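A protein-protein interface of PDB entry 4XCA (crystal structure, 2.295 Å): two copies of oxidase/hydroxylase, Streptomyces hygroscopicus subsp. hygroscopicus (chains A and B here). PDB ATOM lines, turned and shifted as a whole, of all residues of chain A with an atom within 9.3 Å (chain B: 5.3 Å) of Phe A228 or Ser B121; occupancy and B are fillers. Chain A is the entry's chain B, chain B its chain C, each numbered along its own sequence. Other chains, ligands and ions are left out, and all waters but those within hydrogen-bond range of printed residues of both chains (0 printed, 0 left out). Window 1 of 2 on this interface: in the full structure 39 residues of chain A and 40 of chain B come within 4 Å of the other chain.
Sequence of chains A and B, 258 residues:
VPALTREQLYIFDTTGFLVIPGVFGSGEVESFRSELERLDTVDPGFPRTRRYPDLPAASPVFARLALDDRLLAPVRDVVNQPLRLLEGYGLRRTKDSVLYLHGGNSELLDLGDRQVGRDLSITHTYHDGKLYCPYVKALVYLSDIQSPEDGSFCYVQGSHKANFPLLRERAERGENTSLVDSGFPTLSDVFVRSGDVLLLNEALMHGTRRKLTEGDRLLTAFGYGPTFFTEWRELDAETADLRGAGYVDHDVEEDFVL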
ATOM      1  N   VAL A  79      29.043   2.016  35.077  1.00  0.00           N
ATOM      2  CA  VAL A  79      28.999   2.345  33.650  1.00  0.00           C
ATOM      3  C   VAL A  79      29.176   3.855  33.472  1.00  0.00           C
ATOM      4  O   VAL A  79      29.961   4.312  32.632  1.00  0.00           O
ATOM      5  CB  VAL A  79      27.676   1.881  32.994  1.00  0.00           C
ATOM      6  CG1 VAL A  79      27.686   2.136  31.478  1.00  0.00           C
ATOM      7  CG2 VAL A  79      27.450   0.411  33.280  1.00  0.00           C
ATOM      8  N   ASN A  80      28.451   4.622  34.281  1.00  0.00           N
ATOM      9  CA  ASN A  80      28.491   6.078  34.197  1.00  0.00           C
ATOM     10  C   ASN A  80      28.312   6.603  32.753  1.00  0.00           C
ATOM     11  O   ASN A  80      29.037   7.493  32.290  1.00  0.00           O
ATOM     12  CB  ASN A  80      29.794   6.592  34.816  1.00  0.00           C
ATOM     13  CG  ASN A  80      29.764   6.562  36.345  1.00  0.00           C
ATOM     14  OD1 ASN A  80      28.933   7.217  36.966  1.00  0.00           O
ATOM     15  ND2 ASN A  80      30.672   5.800  36.950  1.00  0.00           N
ATOM     16  N   GLN A  81      27.343   6.020  32.052  1.00  0.00           N
ATOM     17  CA  GLN A  81      26.885   6.506  30.743  1.00  0.00           C
ATOM     18  C   GLN A  81      25.359   6.454  30.685  1.00  0.00           C
ATOM     19  O   GLN A  81      24.725   5.762  31.498  1.00  0.00           O
ATOM     20  CB  GLN A  81      27.456   5.651  29.601  1.00  0.00           C
ATOM     21  CG  GLN A  81      28.949   5.636  29.502  1.00  0.00           C
ATOM     22  CD  GLN A  81      29.497   6.849  28.786  1.00  0.00           C
ATOM     23  OE1 GLN A  81      29.573   6.871  27.565  1.00  0.00           O
ATOM     24  NE2 GLN A  81      29.918   7.849  29.545  1.00  0.00           N
ATOM     25  N   PRO A  82      24.755   7.150  29.707  1.00  0.00           N
ATOM     26  CA  PRO A  82      23.323   6.880  29.494  1.00  0.00           C
ATOM     27  C   PRO A  82      23.085   5.394  29.206  1.00  0.00           C
ATOM     28  O   PRO A  82      23.672   4.860  28.267  1.00  0.00           O
ATOM     29  CB  PRO A  82      22.970   7.745  28.279  1.00  0.00           C
ATOM     30  CG  PRO A  82      23.987   8.832  28.270  1.00  0.00           C
ATOM     31  CD  PRO A  82      25.255   8.224  28.831  1.00  0.00           C
ATOM     32  N   LEU A  83      22.249   4.751  30.015  1.00  0.00           N
ATOM     33  CA  LEU A  83      22.051   3.304  29.997  1.00  0.00           C
ATOM     34  C   LEU A  83      20.968   2.786  29.058  1.00  0.00           C
ATOM     35  O   LEU A  83      19.977   3.464  28.781  1.00  0.00           O
ATOM     36  CB  LEU A  83      21.691   2.809  31.404  1.00  0.00           C
ATOM     37  CG  LEU A  83      22.754   2.801  32.491  1.00  0.00           C
ATOM     38  CD1 LEU A  83      22.215   2.165  33.768  1.00  0.00           C
ATOM     39  CD2 LEU A  83      23.962   2.057  31.971  1.00  0.00           C
ATOM     40  N   ARG A  84      21.158   1.553  28.601  1.00  0.00           N
ATOM     41  CA  ARG A  84      20.049   0.753  28.110  1.00  0.00           C
ATOM     42  C   ARG A  84      20.255  -0.713  28.499  1.00  0.00           C
ATOM     43  O   ARG A  84      21.395  -1.162  28.722  1.00  0.00           O
ATOM     44  CB  ARG A  84      19.872   0.916  26.595  1.00  0.00           C
ATOM     45  CG  ARG A  84      20.876   0.226  25.746  1.00  0.00           C
ATOM     46  CD  ARG A  84      20.554   0.358  24.246  1.00  0.00           C
ATOM     47  NE  ARG A  84      19.309  -0.308  23.838  1.00  0.00           N
ATOM     48  CZ  ARG A  84      19.047  -0.720  22.596  1.00  0.00           C
ATOM     49  NH1 ARG A  84      19.942  -0.561  21.631  1.00  0.00           N
ATOM     50  NH2 ARG A  84      17.896  -1.307  22.313  1.00  0.00           N
ATOM     51  N   LEU A  85      19.141  -1.431  28.633  1.00  0.00           N
ATOM     52  CA  LEU A  85      19.148  -2.868  28.895  1.00  0.00           C
ATOM     53  C   LEU A  85      19.562  -3.609  27.630  1.00  0.00           C
ATOM     54  O   LEU A  85      18.909  -3.497  26.593  1.00  0.00           O
ATOM     55  CB  LEU A  85      17.771  -3.324  29.364  1.00  0.00           C
ATOM     56  CG  LEU A  85      17.498  -4.801  29.578  1.00  0.00           C
ATOM     57  CD1 LEU A  85      18.400  -5.324  30.684  1.00  0.00           C
ATOM     58  CD2 LEU A  85      16.019  -5.015  29.929  1.00  0.00           C
ATOM     59  N   LEU A  86      20.659  -4.354  27.698  1.00  0.00           N
ATOM     60  CA  LEU A  86      21.154  -5.033  26.509  1.00  0.00           C
ATOM     61  C   LEU A  86      20.734  -6.496  26.447  1.00  0.00           C
ATOM     62  O   LEU A  86      20.720  -7.079  25.369  1.00  0.00           O
ATOM     63  CB  LEU A  86      22.677  -4.922  26.434  1.00  0.00           C
ATOM     64  CG  LEU A  86      23.258  -3.499  26.391  1.00  0.00           C
ATOM     65  CD1 LEU A  86      24.794  -3.568  26.342  1.00  0.00           C
ATOM     66  CD2 LEU A  86      22.706  -2.689  25.214  1.00  0.00           C
ATOM     67  N   LEU A 120      36.294  -3.695  22.078  1.00  0.00           N
ATOM     68  CA  LEU A 120      35.820  -2.398  22.557  1.00  0.00           C
ATOM     69  C   LEU A 120      34.467  -2.494  23.239  1.00  0.00           C
ATOM     70  O   LEU A 120      34.043  -1.541  23.875  1.00  0.00           O
ATOM     71  CB  LEU A 120      35.748  -1.386  21.410  1.00  0.00           C
ATOM     72  CG  LEU A 120      37.131  -1.090  20.825  1.00  0.00           C
ATOM     73  CD1 LEU A 120      37.095   0.020  19.773  1.00  0.00           C
ATOM     74  CD2 LEU A 120      38.111  -0.753  21.941  1.00  0.00           C
ATOM     75  N   SER A 121      33.786  -3.632  23.110  1.00  0.00           N
ATOM     76  CA  SER A 121      32.501  -3.805  23.793  1.00  0.00           C
ATOM     77  C   SER A 121      32.693  -3.957  25.288  1.00  0.00           C
ATOM     78  O   SER A 121      31.760  -3.709  26.058  1.00  0.00           O
ATOM     79  CB  SER A 121      31.731  -5.017  23.245  1.00  0.00           C
ATOM     80  OG  SER A 121      32.378  -6.226  23.574  1.00  0.00           O
ATOM     81  N   THR A 123      36.020  -2.947  26.668  1.00  0.00           N
ATOM     82  CA  THR A 123      37.194  -2.143  27.012  1.00  0.00           C
ATOM     83  C   THR A 123      36.776  -0.965  27.897  1.00  0.00           C
ATOM     84  O   THR A 123      35.994  -0.106  27.492  1.00  0.00           O
ATOM     85  CB  THR A 123      37.928  -1.662  25.733  1.00  0.00           C
ATOM     86  OG1 THR A 123      38.560  -2.789  25.116  1.00  0.00           O
ATOM     87  CG2 THR A 123      38.993  -0.631  26.054  1.00  0.00           C
ATOM     88  N   TYR A 132      34.329   3.759  34.033  1.00  0.00           N
ATOM     89  CA  TYR A 132      33.553   3.722  32.793  1.00  0.00           C
ATOM     90  C   TYR A 132      33.664   2.344  32.161  1.00  0.00           C
ATOM     91  O   TYR A 132      34.518   2.106  31.310  1.00  0.00           O
ATOM     92  CB  TYR A 132      34.028   4.802  31.817  1.00  0.00           C
ATOM     93  CG  TYR A 132      33.778   6.210  32.310  1.00  0.00           C
ATOM     94  CD1 TYR A 132      34.749   6.898  33.014  1.00  0.00           C
ATOM     95  CD2 TYR A 132      32.557   6.844  32.083  1.00  0.00           C
ATOM     96  CE1 TYR A 132      34.529   8.192  33.473  1.00  0.00           C
ATOM     97  CE2 TYR A 132      32.319   8.133  32.547  1.00  0.00           C
ATOM     98  CZ  TYR A 132      33.313   8.805  33.240  1.00  0.00           C
ATOM     99  OH  TYR A 132      33.100  10.081  33.707  1.00  0.00           O
ATOM    100  N   CYS A 133      32.784   1.443  32.590  1.00  0.00           N
ATOM    101  CA  CYS A 133      32.729   0.085  32.071  1.00  0.00           C
ATOM    102  C   CYS A 133      31.539  -0.055  31.122  1.00  0.00           C
ATOM    103  O   CYS A 133      30.395   0.074  31.553  1.00  0.00           O
ATOM    104  CB  CYS A 133      32.632  -0.909  33.235  1.00  0.00           C
ATOM    105  SG  CYS A 133      33.947  -0.681  34.509  1.00  0.00           S
ATOM    106  N   PRO A 134      31.795  -0.308  29.826  1.00  0.00           N
ATOM    107  CA  PRO A 134      30.714  -0.334  28.826  1.00  0.00           C
ATOM    108  C   PRO A 134      29.774  -1.539  28.905  1.00  0.00           C
ATOM    109  O   PRO A 134      28.689  -1.461  28.332  1.00  0.00           O
ATOM    110  CB  PRO A 134      31.470  -0.354  27.499  1.00  0.00           C
ATOM    111  CG  PRO A 134      32.764  -1.033  27.833  1.00  0.00           C
ATOM    112  CD  PRO A 134      33.113  -0.513  29.207  1.00  0.00           C
ATOM    113  N   TYR A 135      30.172  -2.623  29.574  1.00  0.00           N
ATOM    114  CA  TYR A 135      29.320  -3.811  29.657  1.00  0.00           C
ATOM    115  C   TYR A 135      29.396  -4.463  31.018  1.00  0.00           C
ATOM    116  O   TYR A 135      30.397  -5.103  31.342  1.00  0.00           O
ATOM    117  CB  TYR A 135      29.712  -4.830  28.589  1.00  0.00           C
ATOM    118  CG  TYR A 135      28.583  -5.710  28.097  1.00  0.00           C
ATOM    119  CD1 TYR A 135      27.602  -6.189  28.962  1.00  0.00           C
ATOM    120  CD2 TYR A 135      28.497  -6.055  26.761  1.00  0.00           C
ATOM    121  CE1 TYR A 135      26.579  -6.998  28.505  1.00  0.00           C
ATOM    122  CE2 TYR A 135      27.475  -6.855  26.292  1.00  0.00           C
ATOM    123  CZ  TYR A 135      26.519  -7.323  27.164  1.00  0.00           C
ATOM    124  OH  TYR A 135      25.504  -8.117  26.673  1.00  0.00           O
ATOM    125  N   GLY A 225      24.552  -1.579  29.200  1.00  0.00           N
ATOM    126  CA  GLY A 225      25.613  -0.840  28.546  1.00  0.00           C
ATOM    127  C   GLY A 225      25.088   0.514  28.113  1.00  0.00           C
ATOM    128  O   GLY A 225      23.950   0.874  28.425  1.00  0.00           O
ATOM    129  N   PRO A 226      25.915   1.280  27.389  1.00  0.00           N
ATOM    130  CA  PRO A 226      25.482   2.598  26.926  1.00  0.00           C
ATOM    131  C   PRO A 226      24.354   2.511  25.892  1.00  0.00           C
ATOM    132  O   PRO A 226      24.196   1.485  25.223  1.00  0.00           O
ATOM    133  CB  PRO A 226      26.753   3.181  26.296  1.00  0.00           C
ATOM    134  CG  PRO A 226      27.881   2.362  26.845  1.00  0.00           C
ATOM    135  CD  PRO A 226      27.297   0.990  26.982  1.00  0.00           C
ATOM    136  N   THR A 227      23.603   3.602  25.762  1.00  0.00           N
ATOM    137  CA  THR A 227      22.476   3.689  24.840  1.00  0.00           C
ATOM    138  C   THR A 227      22.876   3.479  23.381  1.00  0.00           C
ATOM    139  O   THR A 227      22.035   3.149  22.545  1.00  0.00           O
ATOM    140  CB  THR A 227      21.764   5.055  24.958  1.00  0.00           C
ATOM    141  OG1 THR A 227      22.678   6.109  24.637  1.00  0.00           O
ATOM    142  CG2 THR A 227      21.206   5.270  26.364  1.00  0.00           C
ATOM    143  N   PHE A 228      24.151   3.671  23.060  1.00  0.00           N
ATOM    144  CA  PHE A 228      24.579   3.459  21.682  1.00  0.00           C
ATOM    145  C   PHE A 228      25.020   2.027  21.404  1.00  0.00           C
ATOM    146  O   PHE A 228      25.296   1.695  20.250  1.00  0.00           O
ATOM    147  CB  PHE A 228      25.700   4.426  21.291  1.00  0.00           C
ATOM    148  CG  PHE A 228      26.781   4.561  22.314  1.00  0.00           C
ATOM    149  CD1 PHE A 228      27.879   3.716  22.296  1.00  0.00           C
ATOM    150  CD2 PHE A 228      26.719   5.556  23.273  1.00  0.00           C
ATOM    151  CE1 PHE A 228      28.887   3.852  23.238  1.00  0.00           C
ATOM    152  CE2 PHE A 228      27.721   5.703  24.208  1.00  0.00           C
ATOM    153  CZ  PHE A 228      28.811   4.847  24.191  1.00  0.00           C
ATOM    154  N   PHE A 229      25.075   1.187  22.436  1.00  0.00           N
ATOM    155  CA  PHE A 229      25.310  -0.246  22.230  1.00  0.00           C
ATOM    156  C   PHE A 229      24.052  -0.943  21.727  1.00  0.00           C
ATOM    157  O   PHE A 229      22.944  -0.652  22.179  1.00  0.00           O
ATOM    158  CB  PHE A 229      25.783  -0.948  23.525  1.00  0.00           C
ATOM    159  CG  PHE A 229      27.289  -0.958  23.717  1.00  0.00           C
ATOM    160  CD1 PHE A 229      28.072   0.127  23.323  1.00  0.00           C
ATOM    161  CD2 PHE A 229      27.915  -2.040  24.311  1.00  0.00           C
ATOM    162  CE1 PHE A 229      29.444   0.128  23.510  1.00  0.00           C
ATOM    163  CE2 PHE A 229      29.288  -2.039  24.503  1.00  0.00           C
ATOM    164  CZ  PHE A 229      30.053  -0.953  24.109  1.00  0.00           C
ATOM    165  N   THR A 230      24.242  -1.883  20.813  1.00  0.00           N
ATOM    166  CA  THR A 230      23.161  -2.699  20.296  1.00  0.00           C
ATOM    167  C   THR A 230      22.810  -3.798  21.317  1.00  0.00           C
ATOM    168  O   THR A 230      23.664  -4.198  22.124  1.00  0.00           O
ATOM    169  CB  THR A 230      23.551  -3.302  18.930  1.00  0.00           C
ATOM    170  OG1 THR A 230      22.378  -3.729  18.232  1.00  0.00           O
ATOM    171  CG2 THR A 230      24.513  -4.472  19.105  1.00  0.00           C
ATOM    172  N   GLU A 231      21.559  -4.259  21.310  1.00  0.00           N
ATOM    173  CA  GLU A 231      21.144  -5.349  22.199  1.00  0.00           C
ATOM    174  C   GLU A 231      21.965  -6.615  21.935  1.00  0.00           C
ATOM    175  O   GLU A 231      22.384  -6.859  20.804  1.00  0.00           O
ATOM    176  CB  GLU A 231      19.658  -5.641  22.031  1.00  0.00           C
ATOM    177  CG  GLU A 231      18.749  -4.891  22.985  1.00  0.00           C
ATOM    178  CD  GLU A 231      17.295  -4.841  22.503  1.00  0.00           C
ATOM    179  OE1 GLU A 231      16.382  -4.935  23.351  1.00  0.00           O
ATOM    180  OE2 GLU A 231      17.065  -4.696  21.280  1.00  0.00           O
ATOM    181  N   TYR A 247      27.673  -8.884  18.634  1.00  0.00           N
ATOM    182  CA  TYR A 247      28.940  -9.026  19.347  1.00  0.00           C
ATOM    183  C   TYR A 247      29.737 -10.243  18.885  1.00  0.00           C
ATOM    184  O   TYR A 247      29.300 -11.381  19.077  1.00  0.00           O
ATOM    185  CB  TYR A 247      28.686  -9.133  20.857  1.00  0.00           C
ATOM    186  CG  TYR A 247      28.043  -7.903  21.455  1.00  0.00           C
ATOM    187  CD1 TYR A 247      28.788  -7.011  22.218  1.00  0.00           C
ATOM    188  CD2 TYR A 247      26.694  -7.626  21.255  1.00  0.00           C
ATOM    189  CE1 TYR A 247      28.215  -5.889  22.766  1.00  0.00           C
ATOM    190  CE2 TYR A 247      26.113  -6.498  21.798  1.00  0.00           C
ATOM    191  CZ  TYR A 247      26.881  -5.624  22.547  1.00  0.00           C
ATOM    192  OH  TYR A 247      26.316  -4.491  23.093  1.00  0.00           O
ATOM    193  N   ASP B 119      32.868   9.915  27.028  1.00  0.00           N
ATOM    194  CA  ASP B 119      31.868   9.399  26.101  1.00  0.00           C
ATOM    195  C   ASP B 119      32.425   8.126  25.494  1.00  0.00           C
ATOM    196  O   ASP B 119      33.342   8.181  24.676  1.00  0.00           O
ATOM    197  CB  ASP B 119      31.563  10.413  24.996  1.00  0.00           C
ATOM    198  CG  ASP B 119      30.347  10.040  24.156  1.00  0.00           C
ATOM    199  OD1 ASP B 119      29.942   8.851  24.136  1.00  0.00           O
ATOM    200  OD2 ASP B 119      29.794  10.959  23.507  1.00  0.00           O
ATOM    201  N   LEU B 120      31.869   6.981  25.874  1.00  0.00           N
ATOM    202  CA  LEU B 120      32.434   5.714  25.439  1.00  0.00           C
ATOM    203  C   LEU B 120      32.241   5.433  23.943  1.00  0.00           C
ATOM    204  O   LEU B 120      32.861   4.515  23.411  1.00  0.00           O
ATOM    205  CB  LEU B 120      31.853   4.567  26.278  1.00  0.00           C
ATOM    206  CG  LEU B 120      32.277   4.577  27.759  1.00  0.00           C
ATOM    207  CD1 LEU B 120      31.855   3.310  28.488  1.00  0.00           C
ATOM    208  CD2 LEU B 120      33.775   4.799  27.906  1.00  0.00           C
ATOM    209  N   SER B 121      31.412   6.214  23.251  1.00  0.00           N
ATOM    210  CA  SER B 121      31.293   6.027  21.803  1.00  0.00           C
ATOM    211  C   SER B 121      32.493   6.592  21.029  1.00  0.00           C
ATOM    212  O   SER B 121      32.678   6.260  19.857  1.00  0.00           O
ATOM    213  CB  SER B 121      29.998   6.654  21.268  1.00  0.00           C
ATOM    214  OG  SER B 121      30.105   8.053  21.207  1.00  0.00           O
ATOM    215  N   ILE B 122      33.305   7.442  21.664  1.00  0.00           N
ATOM    216  CA  ILE B 122      34.497   7.980  20.989  1.00  0.00           C
ATOM    217  C   ILE B 122      35.787   7.682  21.748  1.00  0.00           C
ATOM    218  O   ILE B 122      36.867   8.101  21.336  1.00  0.00           O
ATOM    219  CB  ILE B 122      34.411   9.499  20.794  1.00  0.00           C
ATOM    220  CG1 ILE B 122      34.178  10.167  22.160  1.00  0.00           C
ATOM    221  CG2 ILE B 122      33.321   9.841  19.785  1.00  0.00           C
ATOM    222  CD1 ILE B 122      34.001  11.627  22.113  1.00  0.00           C
ATOM    223  N   THR B 123      35.675   6.959  22.857  1.00  0.00           N
ATOM    224  CA  THR B 123      36.833   6.706  23.691  1.00  0.00           C
ATOM    225  C   THR B 123      37.693   5.626  23.050  1.00  0.00           C
ATOM    226  O   THR B 123      37.319   4.460  22.959  1.00  0.00           O
ATOM    227  CB  THR B 123      36.408   6.354  25.113  1.00  0.00           C
ATOM    228  OG1 THR B 123      35.939   7.558  25.735  1.00  0.00           O
ATOM    229  CG2 THR B 123      37.579   5.787  25.938  1.00  0.00           C
ATOM    230  N   PRO B 134      36.685   3.601  18.184  1.00  0.00           N
ATOM    231  CA  PRO B 134      35.327   3.068  18.024  1.00  0.00           C
ATOM    232  C   PRO B 134      34.445   3.845  17.041  1.00  0.00           C
ATOM    233  O   PRO B 134      33.499   3.265  16.520  1.00  0.00           O
ATOM    234  CB  PRO B 134      34.744   3.158  19.446  1.00  0.00           C
ATOM    235  CG  PRO B 134      35.499   4.241  20.093  1.00  0.00           C
ATOM    236  CD  PRO B 134      36.904   4.126  19.545  1.00  0.00           C
ATOM    237  N   TYR B 135      34.730   5.118  16.792  1.00  0.00           N
ATOM    238  CA  TYR B 135      33.892   5.895  15.886  1.00  0.00           C
ATOM    239  C   TYR B 135      34.740   6.802  15.009  1.00  0.00           C
ATOM    240  O   TYR B 135      35.309   7.787  15.488  1.00  0.00           O
ATOM    241  CB  TYR B 135      32.870   6.714  16.684  1.00  0.00           C
ATOM    242  CG  TYR B 135      31.595   7.004  15.935  1.00  0.00           C
ATOM    243  CD1 TYR B 135      31.623   7.534  14.649  1.00  0.00           C
ATOM    244  CD2 TYR B 135      30.360   6.739  16.508  1.00  0.00           C
ATOM    245  CE1 TYR B 135      30.449   7.800  13.947  1.00  0.00           C
ATOM    246  CE2 TYR B 135      29.173   7.001  15.815  1.00  0.00           C
ATOM    247  CZ  TYR B 135      29.228   7.524  14.535  1.00  0.00           C
ATOM    248  OH  TYR B 135      28.064   7.780  13.845  1.00  0.00           O
ATOM    249  N   PHE B 228      28.821  -3.811  17.217  1.00  0.00           N
ATOM    250  CA  PHE B 228      27.932  -3.698  18.373  1.00  0.00           C
ATOM    251  C   PHE B 228      27.491  -2.252  18.680  1.00  0.00           C
ATOM    252  O   PHE B 228      26.713  -2.032  19.608  1.00  0.00           O
ATOM    253  CB  PHE B 228      28.570  -4.323  19.619  1.00  0.00           C
ATOM    254  CG  PHE B 228      29.977  -3.891  19.877  1.00  0.00           C
ATOM    255  CD1 PHE B 228      30.241  -2.730  20.577  1.00  0.00           C
ATOM    256  CD2 PHE B 228      31.041  -4.667  19.453  1.00  0.00           C
ATOM    257  CE1 PHE B 228      31.551  -2.338  20.832  1.00  0.00           C
ATOM    258  CE2 PHE B 228      32.351  -4.278  19.691  1.00  0.00           C
ATOM    259  CZ  PHE B 228      32.604  -3.111  20.376  1.00  0.00           C
ATOM    260  N   PHE B 229      27.994  -1.276  17.917  1.00  0.00           N
ATOM    261  CA  PHE B 229      27.437   0.083  17.911  1.00  0.00           C
ATOM    262  C   PHE B 229      26.139   0.111  17.076  1.00  0.00           C
ATOM    263  O   PHE B 229      26.057  -0.546  16.037  1.00  0.00           O
ATOM    264  CB  PHE B 229      28.434   1.100  17.318  1.00  0.00           C
ATOM    265  CG  PHE B 229      29.444   1.645  18.298  1.00  0.00           C
ATOM    266  CD1 PHE B 229      30.023   0.828  19.269  1.00  0.00           C
ATOM    267  CD2 PHE B 229      29.855   2.972  18.210  1.00  0.00           C
ATOM    268  CE1 PHE B 229      30.965   1.326  20.161  1.00  0.00           C
ATOM    269  CE2 PHE B 229      30.811   3.483  19.100  1.00  0.00           C
ATOM    270  CZ  PHE B 229      31.357   2.653  20.080  1.00  0.00           C
ATOM    271  N   THR B 230      25.144   0.875  17.515  1.00  0.00           N
ATOM    272  CA  THR B 230      23.933   1.109  16.718  1.00  0.00           C
ATOM    273  C   THR B 230      24.172   2.167  15.628  1.00  0.00           C
ATOM    274  O   THR B 230      25.046   3.011  15.773  1.00  0.00           O
ATOM    275  CB  THR B 230      22.744   1.574  17.616  1.00  0.00           C
ATOM    276  OG1 THR B 230      23.130   2.727  18.374  1.00  0.00           O
ATOM    277  CG2 THR B 230      22.327   0.492  18.583  1.00  0.00           C
ATOM    278  N   GLY B 246      20.537   5.108  21.040  1.00  0.00           N
ATOM    279  CA  GLY B 246      21.000   6.365  20.485  1.00  0.00           C
ATOM    280  C   GLY B 246      22.276   6.883  21.118  1.00  0.00           C
ATOM    281  O   GLY B 246      22.847   6.255  22.014  1.00  0.00           O
ATOM    282  N   TYR B 247      22.700   8.050  20.646  1.00  0.00           N
ATOM    283  CA  TYR B 247      23.920   8.704  21.076  1.00  0.00           C
ATOM    284  C   TYR B 247      23.617  10.019  21.764  1.00  0.00           C
ATOM    285  O   TYR B 247      23.090  10.928  21.133  1.00  0.00           O
ATOM    286  CB  TYR B 247      24.831   8.958  19.877  1.00  0.00           C
ATOM    287  CG  TYR B 247      25.354   7.701  19.227  1.00  0.00           C
ATOM    288  CD1 TYR B 247      26.692   7.350  19.353  1.00  0.00           C
ATOM    289  CD2 TYR B 247      24.515   6.855  18.504  1.00  0.00           C
ATOM    290  CE1 TYR B 247      27.191   6.217  18.764  1.00  0.00           C
ATOM    291  CE2 TYR B 247      25.004   5.708  17.918  1.00  0.00           C
ATOM    292  CZ  TYR B 247      26.352   5.393  18.048  1.00  0.00           C
ATOM    293  OH  TYR B 247      26.878   4.258  17.475  1.00  0.00           O
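Among the printed residues, pairs that only touch across the chains: Ser A121 with Phe B228 (3.0 Å), Phe A228 with Ser B121 (3.1 Å), Phe A228 with Tyr B247 (3.4 Å), Phe A229 with Phe B228 (3.5 Å), Leu A120 with Phe B228 (3.5 Å), Phe A228 with Leu B120 (3.5 Å), Tyr A247 with Phe B228 (3.5 Å), Phe A228 with Phe B229 (3.6 Å), Gln A81 with Asp B119 (3.7 Å), Thr A230 with Thr B230 (3.7 Å), Pro A134 with Leu B120 (3.8 Å), Phe A229 with Thr B230 (3.8 Å), Phe A228 with Asp B119 (3.9 Å), Phe A229 with Phe B229 (3.9 Å), Tyr A132 with Leu B120 (3.9 Å) and Leu A120 with Pro B134 (3.9 Å).
Ser A121 touches Phe B228, and with the chains exchanged Phe A228 touches Ser B121.
Phe A228 touches Thr B230, and with the chains exchanged Thr A230 touches Phe B228.
Phe A228 touches Tyr B247, and with the chains exchanged Tyr A247 touches Phe B228.
Phe A229 touches Thr B230, but with the chains exchanged Thr A230 does not touch Phe B229 (4.6 Å).
Of the 21 pairs that touch across the chains among the printed residues, 14 have their exchanged pair printed and touching as well.
The side-chain hydroxyl of Tyr B247 lies within hydrogen-bond range of the backbone carbonyl oxygen of Thr B230.
O of Pro A82 is in hydrogen-bond range of N of Thr A227 (2.8 Å).
OD1 of Asp B119 is in hydrogen-bond range of OG of Ser B121.
The backbone carbonyl oxygen (O) of Thr A230 lies within hydrogen-bond range of the side-chain hydroxyl (OH) of Tyr A247 (2.8 Å).
The guanidinium group (NH1) of Arg A84 sits at hydrogen-bond distance from the backbone carbonyl oxygen (O) of Phe A229 (3.1 Å).
The side-chain hydroxyl (OG1) of Thr B123 lies within hydrogen-bond range of the backbone carbonyl oxygen (O) of Asp B119 (2.9 Å).
Hydrophobic or aromatic side chains of chain A that line the printed part of chain B: Leu A120, Tyr A132, Pro A134, Phe A228, Phe A229 and Tyr A247.
Hydrophobic or aromatic side chains of chain B that line the printed part of chain A: Leu B120, Pro B134, Phe B228, Phe B229 and Tyr B247.
Among the printed residues, 21 pairs touch across the chains.
Among the printed residues, no Asp or Glu carboxylate lies within 4 Å of a Lys or Arg side-chain nitrogen of the other chain.
Leu A85 touches none of the printed residues of chain B.
Of the printed residues of chain B, Leu A120 touches Pro B134 and Phe B228.
Of the printed residues of chain B, Ser A121 touches Phe B228.
Of the printed residues of chain B, Tyr A132 touches Leu B120 (3.9 Å).
Phe A228 touches just these residues of chain B: Asp B119 (3.9 Å), Leu B120 (3.5 Å), Ser B121 (3.1 Å), Phe B229 (3.6 Å), Thr B230 (2.9 Å), Gly B246 (3.1 Å) and Tyr B247 (3.4 Å).
Of the printed residues of chain A, Leu B120 touches Gln A81 (2.9 Å), Tyr A132 (3.9 Å), Pro A134 (3.8 Å) and Phe A228 (3.5 Å).
Printed residues of chain A within 4 Å of Ser B121: Phe A228.
Pro B134 touches one residue of chain A.
Of chain A, only Phe A228 and Phe A229 come within 4 Å of Phe B229.
Of the printed residues of chain A, Gly B246 touches Thr A227 (2.6 Å) and Phe A228 (3.1 Å).
The nearest residue of chain A that does not touch Ser B121 is Gln A81 (4.7 Å).
The nearest printed residue of chain A that does not touch Leu B120 is Cys A133 (4.3 Å).
The backbone carbonyl oxygen (O) of Phe A228 sits at hydrogen-bond distance from the backbone NH (N) of Thr B230.
The backbone carbonyl oxygen (O) of Gly B246 is in hydrogen-bond range of the backbone NH (N) of Phe A228, at 3.1 Å.
N of Leu B120 sits at hydrogen-bond distance from OE1 of Gln A81.
N of Thr A230 sits at hydrogen-bond distance from O of Phe B228 (2.8 Å).
The side-chain hydroxyl of Thr A227 is in hydrogen-bond range of the backbone carbonyl oxygen of Gly B246.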
